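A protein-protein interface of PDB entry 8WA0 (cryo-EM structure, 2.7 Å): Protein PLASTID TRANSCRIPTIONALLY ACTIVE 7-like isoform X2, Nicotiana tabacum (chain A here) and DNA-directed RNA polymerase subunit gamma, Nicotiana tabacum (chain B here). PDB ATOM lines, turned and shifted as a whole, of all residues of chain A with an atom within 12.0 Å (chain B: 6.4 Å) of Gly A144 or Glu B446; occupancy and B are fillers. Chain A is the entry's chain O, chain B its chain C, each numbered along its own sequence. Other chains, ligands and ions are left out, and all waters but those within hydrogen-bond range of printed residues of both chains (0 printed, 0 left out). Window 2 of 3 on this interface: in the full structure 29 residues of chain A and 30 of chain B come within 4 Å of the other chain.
Hydrophobic or aromatic side chains of chain A that line the printed part of chain B: Leu A146.
Among the printed residues, 6 pairs touch across the chains.
Glu B450 touches Lys A112.
Gly A144 touches Glu B446.
OE2 of Glu B446 touches CG of Leu A146 (3.3 Å).
Leu A146 touches Gln B449.
Of chain B, only Glu B446 (3.4 Å) comes within 4 Å of Gly A144.
No residue of chain A comes within 4 Å of Pro B442.
No residue of chain A comes within 4 Å of Ile B443.
No residue of chain A comes within 4 Å of Ile B447.
Leu B448 touches none of the printed residues of chain A.
Gln B449 touches just one residue of chain A: Leu A146 (3.5 Å).
Of chain A, only Lys A112 (3.9 Å) comes within 4 Å of Glu B450.
Of the printed residues of chain B, Lys A112 touches Glu B450 and Val B451.
Printed residues of chain B within 4 Å of Leu A146: Glu B446 and Gln B449.
Printed residues of chain A within 4 Å of Val B451: Lys A112 (3.1 Å).
Of the printed residues of chain B, Tyr A145 touches Glu B446 (3.4 Å).
Ala A110 touches none of the printed residues of chain B.
Lys A111 touches none of the printed residues of chain B.
The nearest residue of chain A that does not touch Glu B446 is Pro A143 (5.6 Å).
The nearest printed residue of chain B that does not touch Leu A146 is Trp B445 (4.2 Å).
The backbone NH (N) of Tyr A145 sits at hydrogen-bond distance from the side-chain carboxylate (OE2) of Glu B446.
The side-chain amino group (NZ) of Lys A112 is in hydrogen-bond range of the backbone carbonyl oxygen (O) of Val B451.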
ATOM      1  N   GLY A 109     -10.117 -22.586  -5.005  1.00  0.00           N
ATOM      2  CA  GLY A 109     -10.738 -21.354  -4.557  1.00  0.00           C
ATOM      3  C   GLY A 109      -9.795 -20.189  -4.714  1.00  0.00           C
ATOM      4  O   GLY A 109     -10.202 -19.132  -5.159  1.00  0.00           O
ATOM      5  N   ALA A 110      -8.536 -20.358  -4.372  1.00  0.00           N
ATOM      6  CA  ALA A 110      -7.559 -19.337  -4.629  1.00  0.00           C
ATOM      7  C   ALA A 110      -6.648 -19.996  -5.614  1.00  0.00           C
ATOM      8  O   ALA A 110      -5.913 -19.324  -6.316  1.00  0.00           O
ATOM      9  CB  ALA A 110      -6.824 -19.001  -3.383  1.00  0.00           C
ATOM     10  N   LYS A 111      -6.719 -21.307  -5.715  1.00  0.00           N
ATOM     11  CA  LYS A 111      -5.963 -22.028  -6.686  1.00  0.00           C
ATOM     12  C   LYS A 111      -7.031 -22.373  -7.618  1.00  0.00           C
ATOM     13  O   LYS A 111      -8.092 -22.801  -7.214  1.00  0.00           O
ATOM     14  CB  LYS A 111      -5.369 -23.287  -6.105  1.00  0.00           C
ATOM     15  CG  LYS A 111      -4.728 -24.211  -7.119  1.00  0.00           C
ATOM     16  CD  LYS A 111      -4.290 -25.511  -6.473  1.00  0.00           C
ATOM     17  CE  LYS A 111      -3.267 -25.266  -5.388  1.00  0.00           C
ATOM     18  NZ  LYS A 111      -2.884 -26.535  -4.718  1.00  0.00           N
ATOM     19  N   LYS A 112      -6.801 -22.144  -8.879  1.00  0.00           N
ATOM     20  CA  LYS A 112      -7.793 -22.392  -9.861  1.00  0.00           C
ATOM     21  C   LYS A 112      -7.510 -23.665 -10.605  1.00  0.00           C
ATOM     22  O   LYS A 112      -6.380 -23.930 -10.933  1.00  0.00           O
ATOM     23  CB  LYS A 112      -7.835 -21.187 -10.776  1.00  0.00           C
ATOM     24  CG  LYS A 112      -8.008 -19.864 -10.050  1.00  0.00           C
ATOM     25  CD  LYS A 112      -9.444 -19.384 -10.104  1.00  0.00           C
ATOM     26  CE  LYS A 112      -9.743 -18.425  -8.973  1.00  0.00           C
ATOM     27  NZ  LYS A 112      -8.669 -17.420  -8.826  1.00  0.00           N
ATOM     28  N   MET A 134       1.156 -19.828  -9.388  1.00  0.00           N
ATOM     29  CA  MET A 134       0.870 -18.991  -8.257  1.00  0.00           C
ATOM     30  C   MET A 134       2.140 -18.554  -7.615  1.00  0.00           C
ATOM     31  O   MET A 134       2.988 -19.374  -7.302  1.00  0.00           O
ATOM     32  CB  MET A 134      -0.015 -19.744  -7.285  1.00  0.00           C
ATOM     33  CG  MET A 134      -1.031 -18.890  -6.571  1.00  0.00           C
ATOM     34  SD  MET A 134      -2.240 -19.932  -5.749  1.00  0.00           S
ATOM     35  CE  MET A 134      -3.172 -18.698  -4.846  1.00  0.00           C
ATOM     36  N   GLU A 135       2.293 -17.256  -7.425  1.00  0.00           N
ATOM     37  CA  GLU A 135       3.498 -16.721  -6.849  1.00  0.00           C
ATOM     38  C   GLU A 135       3.234 -15.849  -5.654  1.00  0.00           C
ATOM     39  O   GLU A 135       2.324 -15.030  -5.690  1.00  0.00           O
ATOM     40  CB  GLU A 135       4.239 -15.902  -7.890  1.00  0.00           C
ATOM     41  CG  GLU A 135       4.815 -16.712  -9.039  1.00  0.00           C
ATOM     42  CD  GLU A 135       5.948 -17.624  -8.605  1.00  0.00           C
ATOM     43  OE1 GLU A 135       6.685 -17.260  -7.663  1.00  0.00           O
ATOM     44  OE2 GLU A 135       6.112 -18.700  -9.217  1.00  0.00           O
ATOM     45  N   SER A 136       4.017 -16.009  -4.590  1.00  0.00           N
ATOM     46  CA  SER A 136       3.883 -15.163  -3.396  1.00  0.00           C
ATOM     47  C   SER A 136       4.550 -13.796  -3.505  1.00  0.00           C
ATOM     48  O   SER A 136       5.434 -13.624  -4.340  1.00  0.00           O
ATOM     49  CB  SER A 136       4.455 -15.891  -2.194  1.00  0.00           C
ATOM     50  OG  SER A 136       3.805 -17.133  -1.995  1.00  0.00           O
ATOM     51  N   ASP A 137       4.150 -12.819  -2.687  1.00  0.00           N
ATOM     52  CA  ASP A 137       4.824 -11.524  -2.685  1.00  0.00           C
ATOM     53  C   ASP A 137       5.820 -11.529  -1.582  1.00  0.00           C
ATOM     54  O   ASP A 137       5.463 -11.451  -0.418  1.00  0.00           O
ATOM     55  CB  ASP A 137       3.879 -10.353  -2.505  1.00  0.00           C
ATOM     56  CG  ASP A 137       3.011 -10.112  -3.719  1.00  0.00           C
ATOM     57  OD1 ASP A 137       3.178 -10.833  -4.727  1.00  0.00           O
ATOM     58  OD2 ASP A 137       2.160  -9.200  -3.670  1.00  0.00           O
ATOM     59  N   PHE A 139       7.870  -9.321  -0.510  1.00  0.00           N
ATOM     60  CA  PHE A 139       8.025  -8.092   0.258  1.00  0.00           C
ATOM     61  C   PHE A 139       6.816  -7.378   0.853  1.00  0.00           C
ATOM     62  O   PHE A 139       6.905  -6.223   1.176  1.00  0.00           O
ATOM     63  CB  PHE A 139       8.796  -7.112  -0.596  1.00  0.00           C
ATOM     64  CG  PHE A 139       9.993  -7.692  -1.272  1.00  0.00           C
ATOM     65  CD1 PHE A 139      11.067  -8.142  -0.539  1.00  0.00           C
ATOM     66  CD2 PHE A 139      10.050  -7.758  -2.643  1.00  0.00           C
ATOM     67  CE1 PHE A 139      12.171  -8.672  -1.167  1.00  0.00           C
ATOM     68  CE2 PHE A 139      11.149  -8.283  -3.278  1.00  0.00           C
ATOM     69  CZ  PHE A 139      12.213  -8.740  -2.540  1.00  0.00           C
ATOM     70  N   LYS A 140       5.705  -8.056   1.025  1.00  0.00           N
ATOM     71  CA  LYS A 140       4.516  -7.422   1.531  1.00  0.00           C
ATOM     72  C   LYS A 140       4.746  -6.965   2.903  1.00  0.00           C
ATOM     73  O   LYS A 140       5.320  -7.669   3.709  1.00  0.00           O
ATOM     74  CB  LYS A 140       3.305  -8.322   1.474  1.00  0.00           C
ATOM     75  N   PRO A 141       4.268  -5.783   3.200  1.00  0.00           N
ATOM     76  CA  PRO A 141       4.548  -5.213   4.487  1.00  0.00           C
ATOM     77  C   PRO A 141       3.999  -6.004   5.664  1.00  0.00           C
ATOM     78  O   PRO A 141       4.692  -6.148   6.657  1.00  0.00           O
ATOM     79  CB  PRO A 141       3.925  -3.856   4.350  1.00  0.00           C
ATOM     80  N   GLY A 142       2.789  -6.519   5.566  1.00  0.00           N
ATOM     81  CA  GLY A 142       2.189  -7.260   6.655  1.00  0.00           C
ATOM     82  C   GLY A 142       0.828  -7.779   6.268  1.00  0.00           C
ATOM     83  O   GLY A 142       0.424  -7.625   5.120  1.00  0.00           O
ATOM     84  N   PRO A 143       0.108  -8.396   7.201  1.00  0.00           N
ATOM     85  CA  PRO A 143      -1.261  -8.841   6.920  1.00  0.00           C
ATOM     86  C   PRO A 143      -2.182  -7.681   6.659  1.00  0.00           C
ATOM     87  O   PRO A 143      -2.029  -6.631   7.277  1.00  0.00           O
ATOM     88  CB  PRO A 143      -1.686  -9.511   8.210  1.00  0.00           C
ATOM     89  CG  PRO A 143      -0.746  -9.018   9.261  1.00  0.00           C
ATOM     90  CD  PRO A 143       0.547  -8.763   8.555  1.00  0.00           C
ATOM     91  N   GLY A 144      -3.113  -7.855   5.731  1.00  0.00           N
ATOM     92  CA  GLY A 144      -4.043  -6.795   5.409  1.00  0.00           C
ATOM     93  C   GLY A 144      -3.402  -5.625   4.709  1.00  0.00           C
ATOM     94  O   GLY A 144      -3.810  -4.499   4.935  1.00  0.00           O
ATOM     95  N   TYR A 145      -2.437  -5.892   3.826  1.00  0.00           N
ATOM     96  CA  TYR A 145      -1.798  -4.838   3.035  1.00  0.00           C
ATOM     97  C   TYR A 145      -1.938  -5.132   1.545  1.00  0.00           C
ATOM     98  O   TYR A 145      -1.728  -6.260   1.119  1.00  0.00           O
ATOM     99  CB  TYR A 145      -0.348  -4.681   3.445  1.00  0.00           C
ATOM    100  CG  TYR A 145      -0.149  -3.583   4.445  1.00  0.00           C
ATOM    101  CD1 TYR A 145      -0.194  -2.260   4.056  1.00  0.00           C
ATOM    102  CD2 TYR A 145       0.066  -3.866   5.781  1.00  0.00           C
ATOM    103  CE1 TYR A 145      -0.021  -1.240   4.964  1.00  0.00           C
ATOM    104  CE2 TYR A 145       0.241  -2.854   6.699  1.00  0.00           C
ATOM    105  CZ  TYR A 145       0.195  -1.543   6.281  1.00  0.00           C
ATOM    106  OH  TYR A 145       0.366  -0.525   7.183  1.00  0.00           O
ATOM    107  N   LEU A 146      -2.288  -4.133   0.746  1.00  0.00           N
ATOM    108  CA  LEU A 146      -2.548  -4.370  -0.674  1.00  0.00           C
ATOM    109  C   LEU A 146      -1.671  -3.607  -1.645  1.00  0.00           C
ATOM    110  O   LEU A 146      -1.531  -2.398  -1.531  1.00  0.00           O
ATOM    111  CB  LEU A 146      -3.986  -3.975  -0.970  1.00  0.00           C
ATOM    112  CG  LEU A 146      -5.023  -5.088  -1.007  1.00  0.00           C
ATOM    113  CD1 LEU A 146      -6.200  -4.735  -1.900  1.00  0.00           C
ATOM    114  CD2 LEU A 146      -4.356  -6.369  -1.459  1.00  0.00           C
ATOM    115  N   LYS A 147      -1.121  -4.301  -2.635  1.00  0.00           N
ATOM    116  CA  LYS A 147      -0.256  -3.654  -3.610  1.00  0.00           C
ATOM    117  C   LYS A 147      -1.033  -2.832  -4.602  1.00  0.00           C
ATOM    118  O   LYS A 147      -2.090  -3.256  -5.045  1.00  0.00           O
ATOM    119  CB  LYS A 147       0.586  -4.678  -4.354  1.00  0.00           C
ATOM    120  N   ASP A 148      -0.516  -1.672  -4.974  1.00  0.00           N
ATOM    121  CA  ASP A 148      -1.175  -0.789  -5.897  1.00  0.00           C
ATOM    122  C   ASP A 148      -0.582  -0.957  -7.253  1.00  0.00           C
ATOM    123  O   ASP A 148       0.414  -0.316  -7.568  1.00  0.00           O
ATOM    124  CB  ASP A 148      -1.006   0.637  -5.443  1.00  0.00           C
ATOM    125  N   GLU A 149      -1.166  -1.820  -8.075  1.00  0.00           N
ATOM    126  CA  GLU A 149      -0.575  -2.124  -9.377  1.00  0.00           C
ATOM    127  C   GLU A 149      -0.934  -1.161 -10.479  1.00  0.00           C
ATOM    128  O   GLU A 149      -1.070  -1.584 -11.617  1.00  0.00           O
ATOM    129  CB  GLU A 149      -0.948  -3.536  -9.803  1.00  0.00           C
ATOM    130  CG  GLU A 149      -0.669  -4.584  -8.748  1.00  0.00           C
ATOM    131  CD  GLU A 149      -0.971  -5.975  -9.247  1.00  0.00           C
ATOM    132  OE1 GLU A 149      -1.228  -6.117 -10.458  1.00  0.00           O
ATOM    133  OE2 GLU A 149      -0.950  -6.918  -8.433  1.00  0.00           O
ATOM    134  N   PRO B 442     -11.002  -4.316   6.460  1.00  0.00           N
ATOM    135  CA  PRO B 442      -9.869  -4.512   5.551  1.00  0.00           C
ATOM    136  C   PRO B 442      -9.684  -5.929   4.997  1.00  0.00           C
ATOM    137  O   PRO B 442      -9.178  -6.071   3.890  1.00  0.00           O
ATOM    138  CB  PRO B 442      -8.674  -4.071   6.389  1.00  0.00           C
ATOM    139  CG  PRO B 442      -9.247  -3.142   7.396  1.00  0.00           C
ATOM    140  CD  PRO B 442     -10.585  -3.723   7.735  1.00  0.00           C
ATOM    141  N   ILE B 443     -10.050  -6.955   5.743  1.00  0.00           N
ATOM    142  CA  ILE B 443      -9.893  -8.336   5.309  1.00  0.00           C
ATOM    143  C   ILE B 443     -10.683  -8.633   4.039  1.00  0.00           C
ATOM    144  O   ILE B 443     -10.262  -9.439   3.230  1.00  0.00           O
ATOM    145  CB  ILE B 443     -10.315  -9.294   6.437  1.00  0.00           C
ATOM    146  CG1 ILE B 443     -10.188 -10.763   6.026  1.00  0.00           C
ATOM    147  CG2 ILE B 443     -11.727  -8.988   6.913  1.00  0.00           C
ATOM    148  CD1 ILE B 443      -8.763 -11.254   5.915  1.00  0.00           C
ATOM    149  N   VAL B 444     -11.812  -7.984   3.838  1.00  0.00           N
ATOM    150  CA  VAL B 444     -12.634  -8.279   2.691  1.00  0.00           C
ATOM    151  C   VAL B 444     -11.833  -8.020   1.449  1.00  0.00           C
ATOM    152  O   VAL B 444     -11.894  -8.786   0.514  1.00  0.00           O
ATOM    153  CB  VAL B 444     -13.913  -7.449   2.713  1.00  0.00           C
ATOM    154  CG1 VAL B 444     -14.662  -7.552   1.401  1.00  0.00           C
ATOM    155  CG2 VAL B 444     -14.800  -7.877   3.862  1.00  0.00           C
ATOM    156  N   TRP B 445     -10.913  -7.099   1.547  1.00  0.00           N
ATOM    157  CA  TRP B 445     -10.109  -6.745   0.416  1.00  0.00           C
ATOM    158  C   TRP B 445      -9.041  -7.721   0.093  1.00  0.00           C
ATOM    159  O   TRP B 445      -8.748  -7.915  -1.070  1.00  0.00           O
ATOM    160  CB  TRP B 445      -9.590  -5.338   0.543  1.00  0.00           C
ATOM    161  CG  TRP B 445     -10.634  -4.291   0.742  1.00  0.00           C
ATOM    162  CD1 TRP B 445     -10.767  -3.483   1.822  1.00  0.00           C
ATOM    163  CD2 TRP B 445     -11.687  -3.926  -0.159  1.00  0.00           C
ATOM    164  NE1 TRP B 445     -11.832  -2.644   1.660  1.00  0.00           N
ATOM    165  CE2 TRP B 445     -12.416  -2.897   0.451  1.00  0.00           C
ATOM    166  CE3 TRP B 445     -12.088  -4.376  -1.417  1.00  0.00           C
ATOM    167  CZ2 TRP B 445     -13.513  -2.306  -0.150  1.00  0.00           C
ATOM    168  CZ3 TRP B 445     -13.179  -3.789  -2.007  1.00  0.00           C
ATOM    169  CH2 TRP B 445     -13.880  -2.765  -1.375  1.00  0.00           C
ATOM    170  N   GLU B 446      -8.437  -8.358   1.066  1.00  0.00           N
ATOM    171  CA  GLU B 446      -7.486  -9.414   0.785  1.00  0.00           C
ATOM    172  C   GLU B 446      -8.132 -10.618   0.160  1.00  0.00           C
ATOM    173  O   GLU B 446      -7.567 -11.222  -0.728  1.00  0.00           O
ATOM    174  CB  GLU B 446      -6.711  -9.781   2.016  1.00  0.00           C
ATOM    175  CG  GLU B 446      -6.114  -8.588   2.738  1.00  0.00           C
ATOM    176  CD  GLU B 446      -5.120  -7.811   1.893  1.00  0.00           C
ATOM    177  OE1 GLU B 446      -4.287  -8.443   1.209  1.00  0.00           O
ATOM    178  OE2 GLU B 446      -5.163  -6.564   1.928  1.00  0.00           O
ATOM    179  N   ILE B 447      -9.313 -10.974   0.605  1.00  0.00           N
ATOM    180  CA  ILE B 447     -10.020 -12.059  -0.007  1.00  0.00           C
ATOM    181  C   ILE B 447     -10.429 -11.725  -1.447  1.00  0.00           C
ATOM    182  O   ILE B 447     -10.269 -12.568  -2.316  1.00  0.00           O
ATOM    183  CB  ILE B 447     -11.177 -12.563   0.862  1.00  0.00           C
ATOM    184  CG1 ILE B 447     -10.643 -12.985   2.219  1.00  0.00           C
ATOM    185  CG2 ILE B 447     -11.898 -13.722   0.204  1.00  0.00           C
ATOM    186  CD1 ILE B 447     -11.683 -13.605   3.119  1.00  0.00           C
ATOM    187  N   LEU B 448     -10.914 -10.527  -1.739  1.00  0.00           N
ATOM    188  CA  LEU B 448     -11.303 -10.178  -3.084  1.00  0.00           C
ATOM    189  C   LEU B 448     -10.163 -10.318  -4.027  1.00  0.00           C
ATOM    190  O   LEU B 448     -10.331 -10.802  -5.121  1.00  0.00           O
ATOM    191  CB  LEU B 448     -11.869  -8.765  -3.159  1.00  0.00           C
ATOM    192  CG  LEU B 448     -12.351  -8.184  -4.489  1.00  0.00           C
ATOM    193  CD1 LEU B 448     -13.408  -9.043  -5.153  1.00  0.00           C
ATOM    194  CD2 LEU B 448     -12.870  -6.776  -4.303  1.00  0.00           C
ATOM    195  N   GLN B 449      -8.988  -9.908  -3.611  1.00  0.00           N
ATOM    196  CA  GLN B 449      -7.848  -9.973  -4.472  1.00  0.00           C
ATOM    197  C   GLN B 449      -7.489 -11.360  -4.817  1.00  0.00           C
ATOM    198  O   GLN B 449      -7.067 -11.620  -5.917  1.00  0.00           O
ATOM    199  CB  GLN B 449      -6.651  -9.288  -3.876  1.00  0.00           C
ATOM    200  CG  GLN B 449      -6.401  -7.900  -4.421  1.00  0.00           C
ATOM    201  CD  GLN B 449      -4.930  -7.637  -4.650  1.00  0.00           C
ATOM    202  OE1 GLN B 449      -4.088  -8.491  -4.376  1.00  0.00           O
ATOM    203  NE2 GLN B 449      -4.611  -6.455  -5.163  1.00  0.00           N
ATOM    204  N   GLU B 450      -7.589 -12.255  -3.862  1.00  0.00           N
ATOM    205  CA  GLU B 450      -7.280 -13.644  -4.102  1.00  0.00           C
ATOM    206  C   GLU B 450      -8.199 -14.327  -5.060  1.00  0.00           C
ATOM    207  O   GLU B 450      -7.743 -15.000  -5.939  1.00  0.00           O
ATOM    208  CB  GLU B 450      -7.248 -14.358  -2.777  1.00  0.00           C
ATOM    209  CG  GLU B 450      -6.100 -13.904  -1.907  1.00  0.00           C
ATOM    210  CD  GLU B 450      -4.781 -13.942  -2.650  1.00  0.00           C
ATOM    211  OE1 GLU B 450      -4.458 -14.998  -3.233  1.00  0.00           O
ATOM    212  OE2 GLU B 450      -4.065 -12.916  -2.650  1.00  0.00           O
ATOM    213  N   VAL B 451      -9.483 -14.099  -4.946  1.00  0.00           N
ATOM    214  CA  VAL B 451     -10.484 -14.674  -5.798  1.00  0.00           C
ATOM    215  C   VAL B 451     -10.383 -14.300  -7.261  1.00  0.00           C
ATOM    216  O   VAL B 451     -10.647 -15.125  -8.106  1.00  0.00           O
ATOM    217  CB  VAL B 451     -11.845 -14.290  -5.215  1.00  0.00           C
ATOM    218  CG1 VAL B 451     -12.934 -14.213  -6.260  1.00  0.00           C
ATOM    219  CG2 VAL B 451     -12.207 -15.192  -4.055  1.00  0.00           C
